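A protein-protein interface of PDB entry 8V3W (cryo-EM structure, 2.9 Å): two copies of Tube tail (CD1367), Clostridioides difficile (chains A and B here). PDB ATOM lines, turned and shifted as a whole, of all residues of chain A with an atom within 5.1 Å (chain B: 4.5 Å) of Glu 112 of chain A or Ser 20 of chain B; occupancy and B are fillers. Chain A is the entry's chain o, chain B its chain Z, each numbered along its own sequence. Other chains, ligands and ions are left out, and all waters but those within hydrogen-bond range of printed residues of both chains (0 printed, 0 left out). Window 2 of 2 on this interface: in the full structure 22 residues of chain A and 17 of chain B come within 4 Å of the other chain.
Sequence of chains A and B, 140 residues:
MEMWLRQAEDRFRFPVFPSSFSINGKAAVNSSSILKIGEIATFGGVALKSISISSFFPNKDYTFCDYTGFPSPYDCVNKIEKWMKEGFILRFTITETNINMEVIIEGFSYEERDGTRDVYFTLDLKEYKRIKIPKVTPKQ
The side-chain hydroxyl (OH) of Tyr 74 of chain A sits at hydrogen-bond distance from the side-chain carboxylate (OE2) of Glu 112 of chain A (2.9 Å). OE2 of Glu 111 of chain A is in salt-bridge range of NH1 of Arg 113 of chain A, 3.7 Å away. The guanidinium group of Arg 117 of chain A lies within salt-bridge range of the side-chain carboxylate of Glu 112 of chain A, 3.3 Å away.
Along chain A the printed residues that touch a printed residue of chain B span positions 74 to 117. Hydrophobic or aromatic side chains of chain B within 4 Å of the printed part of chain A: Met 1 and Phe 21.
Of the printed residues of chain B, Tyr 74 of chain A touches Thr 97. Of the printed residues of chain B, Glu 111 of chain A touches Phe 21 (3.2 Å). Ser 20 of chain B touches just one residue of chain A: Glu 112 (3.3 Å). Of the printed residues of chain A, Thr 97 of chain B touches Tyr 74 (3.3 Å). The nearest residue of chain A that does not touch Ser 20 of chain B is Arg 113 of chain A (4.03 Å). The nearest printed residue of chain A that does not touch Met 1 of chain B is Glu 112 of chain A (4.4 Å).
No position is printed for both chains. Of the 5 pairs that touch across the chains among the printed residues, none has its exchanged pair printed and touching as well.
Among the printed residues, pairs that only touch across the chains: Tyr 74 of chain A with Thr 97 of chain B (3.3 Å), Glu 111 of chain A with Phe 21 of chain B (3.2 Å), Glu 112 of chain A with Ser 20 of chain B (3.3 Å) and Arg 117 of chain A with Met 1 of chain B (3.9 Å).
The backbone carbonyl oxygen (O) of Phe 21 of chain B lies within hydrogen-bond range of the backbone NH (N) of Glu 112 of chain A, 3.3 Å away.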
ATOM      1  N   TYR A  74      -4.844   0.334  -9.911  1.00  0.00           N
ATOM      2  CA  TYR A  74      -4.551   0.537 -11.320  1.00  0.00           C
ATOM      3  C   TYR A  74      -3.069   0.751 -11.586  1.00  0.00           C
ATOM      4  O   TYR A  74      -2.625   0.514 -12.710  1.00  0.00           O
ATOM      5  CB  TYR A  74      -5.399   1.685 -11.864  1.00  0.00           C
ATOM      6  CG  TYR A  74      -6.818   1.233 -12.107  1.00  0.00           C
ATOM      7  CD1 TYR A  74      -7.106   0.307 -13.094  1.00  0.00           C
ATOM      8  CD2 TYR A  74      -7.861   1.689 -11.319  1.00  0.00           C
ATOM      9  CE1 TYR A  74      -8.386  -0.133 -13.306  1.00  0.00           C
ATOM     10  CE2 TYR A  74      -9.150   1.254 -11.526  1.00  0.00           C
ATOM     11  CZ  TYR A  74      -9.406   0.346 -12.523  1.00  0.00           C
ATOM     12  OH  TYR A  74     -10.683  -0.094 -12.737  1.00  0.00           O
ATOM     13  N   TYR A 110      -9.032  -8.240 -15.864  1.00  0.00           N
ATOM     14  CA  TYR A 110      -9.400  -7.596 -14.613  1.00  0.00           C
ATOM     15  C   TYR A 110     -10.792  -6.992 -14.731  1.00  0.00           C
ATOM     16  O   TYR A 110     -11.284  -6.736 -15.830  1.00  0.00           O
ATOM     17  CB  TYR A 110      -8.382  -6.527 -14.204  1.00  0.00           C
ATOM     18  CG  TYR A 110      -8.025  -5.539 -15.286  1.00  0.00           C
ATOM     19  CD1 TYR A 110      -7.107  -5.857 -16.273  1.00  0.00           C
ATOM     20  CD2 TYR A 110      -8.589  -4.275 -15.307  1.00  0.00           C
ATOM     21  CE1 TYR A 110      -6.778  -4.953 -17.250  1.00  0.00           C
ATOM     22  CE2 TYR A 110      -8.264  -3.370 -16.281  1.00  0.00           C
ATOM     23  CZ  TYR A 110      -7.358  -3.713 -17.249  1.00  0.00           C
ATOM     24  OH  TYR A 110      -7.026  -2.810 -18.228  1.00  0.00           O
ATOM     25  N   GLU A 111     -11.427  -6.764 -13.582  1.00  0.00           N
ATOM     26  CA  GLU A 111     -12.809  -6.306 -13.574  1.00  0.00           C
ATOM     27  C   GLU A 111     -13.153  -5.650 -12.245  1.00  0.00           C
ATOM     28  O   GLU A 111     -12.434  -5.788 -11.255  1.00  0.00           O
ATOM     29  CB  GLU A 111     -13.768  -7.461 -13.846  1.00  0.00           C
ATOM     30  CG  GLU A 111     -13.780  -8.521 -12.782  1.00  0.00           C
ATOM     31  CD  GLU A 111     -15.129  -9.183 -12.670  1.00  0.00           C
ATOM     32  OE1 GLU A 111     -16.111  -8.590 -13.154  1.00  0.00           O
ATOM     33  OE2 GLU A 111     -15.210 -10.292 -12.106  1.00  0.00           O
ATOM     34  N   GLU A 112     -14.273  -4.929 -12.246  1.00  0.00           N
ATOM     35  CA  GLU A 112     -14.880  -4.359 -11.051  1.00  0.00           C
ATOM     36  C   GLU A 112     -16.319  -4.845 -10.969  1.00  0.00           C
ATOM     37  O   GLU A 112     -17.021  -4.874 -11.982  1.00  0.00           O
ATOM     38  CB  GLU A 112     -14.842  -2.829 -11.077  1.00  0.00           C
ATOM     39  CG  GLU A 112     -13.467  -2.237 -10.861  1.00  0.00           C
ATOM     40  CD  GLU A 112     -13.520  -0.849 -10.263  1.00  0.00           C
ATOM     41  OE1 GLU A 112     -14.293  -0.640  -9.310  1.00  0.00           O
ATOM     42  OE2 GLU A 112     -12.781   0.032 -10.738  1.00  0.00           O
ATOM     43  N   ARG A 113     -16.758  -5.245  -9.771  1.00  0.00           N
ATOM     44  CA  ARG A 113     -18.074  -5.867  -9.671  1.00  0.00           C
ATOM     45  C   ARG A 113     -18.845  -5.524  -8.397  1.00  0.00           C
ATOM     46  O   ARG A 113     -19.798  -6.233  -8.066  1.00  0.00           O
ATOM     47  CB  ARG A 113     -17.951  -7.383  -9.768  1.00  0.00           C
ATOM     48  CG  ARG A 113     -17.140  -7.979  -8.655  1.00  0.00           C
ATOM     49  CD  ARG A 113     -16.703  -9.378  -8.979  1.00  0.00           C
ATOM     50  NE  ARG A 113     -16.553 -10.167  -7.766  1.00  0.00           N
ATOM     51  CZ  ARG A 113     -15.878 -11.304  -7.695  1.00  0.00           C
ATOM     52  NH1 ARG A 113     -15.288 -11.822  -8.759  1.00  0.00           N
ATOM     53  NH2 ARG A 113     -15.791 -11.933  -6.528  1.00  0.00           N
ATOM     54  N   ASP A 114     -18.469  -4.481  -7.665  1.00  0.00           N
ATOM     55  CA  ASP A 114     -19.250  -4.058  -6.505  1.00  0.00           C
ATOM     56  C   ASP A 114     -18.944  -2.593  -6.220  1.00  0.00           C
ATOM     57  O   ASP A 114     -18.365  -1.889  -7.052  1.00  0.00           O
ATOM     58  CB  ASP A 114     -18.986  -4.951  -5.286  1.00  0.00           C
ATOM     59  CG  ASP A 114     -17.513  -5.110  -4.976  1.00  0.00           C
ATOM     60  OD1 ASP A 114     -16.679  -4.422  -5.597  1.00  0.00           O
ATOM     61  OD2 ASP A 114     -17.187  -5.932  -4.100  1.00  0.00           O
ATOM     62  N   ARG A 117     -14.638  -0.550  -5.126  1.00  0.00           N
ATOM     63  CA  ARG A 117     -13.549  -0.133  -6.010  1.00  0.00           C
ATOM     64  C   ARG A 117     -12.345  -1.071  -5.957  1.00  0.00           C
ATOM     65  O   ARG A 117     -11.239  -0.679  -6.329  1.00  0.00           O
ATOM     66  CB  ARG A 117     -13.096   1.303  -5.721  1.00  0.00           C
ATOM     67  CG  ARG A 117     -14.214   2.326  -5.639  1.00  0.00           C
ATOM     68  CD  ARG A 117     -14.920   2.519  -6.972  1.00  0.00           C
ATOM     69  NE  ARG A 117     -14.018   2.441  -8.112  1.00  0.00           N
ATOM     70  CZ  ARG A 117     -13.313   3.458  -8.584  1.00  0.00           C
ATOM     71  NH1 ARG A 117     -13.390   4.660  -8.043  1.00  0.00           N
ATOM     72  NH2 ARG A 117     -12.512   3.262  -9.626  1.00  0.00           N
ATOM     73  N   ASP A 118     -12.529  -2.309  -5.508  1.00  0.00           N
ATOM     74  CA  ASP A 118     -11.478  -3.311  -5.597  1.00  0.00           C
ATOM     75  C   ASP A 118     -11.458  -3.925  -6.992  1.00  0.00           C
ATOM     76  O   ASP A 118     -12.497  -4.084  -7.631  1.00  0.00           O
ATOM     77  CB  ASP A 118     -11.686  -4.405  -4.551  1.00  0.00           C
ATOM     78  CG  ASP A 118     -11.590  -3.888  -3.131  1.00  0.00           C
ATOM     79  OD1 ASP A 118     -10.846  -2.920  -2.886  1.00  0.00           O
ATOM     80  OD2 ASP A 118     -12.260  -4.455  -2.250  1.00  0.00           O
ATOM     81  N   VAL A 119     -10.264  -4.280  -7.459  1.00  0.00           N
ATOM     82  CA  VAL A 119     -10.063  -4.803  -8.807  1.00  0.00           C
ATOM     83  C   VAL A 119      -9.726  -6.285  -8.722  1.00  0.00           C
ATOM     84  O   VAL A 119      -8.673  -6.655  -8.195  1.00  0.00           O
ATOM     85  CB  VAL A 119      -8.959  -4.040  -9.553  1.00  0.00           C
ATOM     86  CG1 VAL A 119      -8.703  -4.669 -10.904  1.00  0.00           C
ATOM     87  CG2 VAL A 119      -9.335  -2.590  -9.712  1.00  0.00           C
ATOM     88  N   MET B   1     -18.514   6.817 -11.214  1.00  0.00           N
ATOM     89  CA  MET B   1     -17.893   6.693 -12.523  1.00  0.00           C
ATOM     90  C   MET B   1     -18.896   6.954 -13.634  1.00  0.00           C
ATOM     91  O   MET B   1     -20.096   6.770 -13.454  1.00  0.00           O
ATOM     92  CB  MET B   1     -17.277   5.305 -12.698  1.00  0.00           C
ATOM     93  CG  MET B   1     -16.298   4.913 -11.617  1.00  0.00           C
ATOM     94  SD  MET B   1     -15.797   3.192 -11.739  1.00  0.00           S
ATOM     95  CE  MET B   1     -17.081   2.401 -10.788  1.00  0.00           C
ATOM     96  N   PRO B  18     -23.614   0.133 -15.741  1.00  0.00           N
ATOM     97  CA  PRO B  18     -23.818  -1.316 -15.646  1.00  0.00           C
ATOM     98  C   PRO B  18     -23.400  -1.873 -14.293  1.00  0.00           C
ATOM     99  O   PRO B  18     -22.798  -1.203 -13.455  1.00  0.00           O
ATOM    100  CB  PRO B  18     -22.936  -1.865 -16.766  1.00  0.00           C
ATOM    101  CG  PRO B  18     -21.893  -0.844 -16.936  1.00  0.00           C
ATOM    102  CD  PRO B  18     -22.552   0.472 -16.695  1.00  0.00           C
ATOM    103  N   SER B  19     -23.743  -3.143 -14.096  1.00  0.00           N
ATOM    104  CA  SER B  19     -23.450  -3.822 -12.841  1.00  0.00           C
ATOM    105  C   SER B  19     -21.989  -4.239 -12.726  1.00  0.00           C
ATOM    106  O   SER B  19     -21.458  -4.297 -11.614  1.00  0.00           O
ATOM    107  CB  SER B  19     -24.364  -5.035 -12.692  1.00  0.00           C
ATOM    108  OG  SER B  19     -24.230  -5.621 -11.417  1.00  0.00           O
ATOM    109  N   SER B  20     -21.329  -4.538 -13.842  1.00  0.00           N
ATOM    110  CA  SER B  20     -19.911  -4.871 -13.823  1.00  0.00           C
ATOM    111  C   SER B  20     -19.331  -4.670 -15.215  1.00  0.00           C
ATOM    112  O   SER B  20     -20.063  -4.581 -16.202  1.00  0.00           O
ATOM    113  CB  SER B  20     -19.682  -6.306 -13.341  1.00  0.00           C
ATOM    114  OG  SER B  20     -19.961  -7.242 -14.361  1.00  0.00           O
ATOM    115  N   PHE B  21     -18.002  -4.594 -15.279  1.00  0.00           N
ATOM    116  CA  PHE B  21     -17.281  -4.485 -16.541  1.00  0.00           C
ATOM    117  C   PHE B  21     -15.944  -5.199 -16.407  1.00  0.00           C
ATOM    118  O   PHE B  21     -15.328  -5.160 -15.343  1.00  0.00           O
ATOM    119  CB  PHE B  21     -17.070  -3.019 -16.948  1.00  0.00           C
ATOM    120  CG  PHE B  21     -16.303  -2.204 -15.942  1.00  0.00           C
ATOM    121  CD1 PHE B  21     -14.924  -2.128 -15.994  1.00  0.00           C
ATOM    122  CD2 PHE B  21     -16.965  -1.494 -14.959  1.00  0.00           C
ATOM    123  CE1 PHE B  21     -14.219  -1.380 -15.077  1.00  0.00           C
ATOM    124  CE2 PHE B  21     -16.262  -0.743 -14.038  1.00  0.00           C
ATOM    125  CZ  PHE B  21     -14.887  -0.686 -14.100  1.00  0.00           C
ATOM    126  N   THR B  97     -10.795   5.204 -14.064  1.00  0.00           N
ATOM    127  CA  THR B  97     -10.039   3.985 -14.329  1.00  0.00           C
ATOM    128  C   THR B  97      -8.941   4.268 -15.343  1.00  0.00           C
ATOM    129  O   THR B  97      -8.677   5.427 -15.667  1.00  0.00           O
ATOM    130  CB  THR B  97     -10.943   2.859 -14.840  1.00  0.00           C
ATOM    131  OG1 THR B  97     -11.418   3.177 -16.149  1.00  0.00           O
ATOM    132  CG2 THR B  97     -12.122   2.645 -13.915  1.00  0.00           C
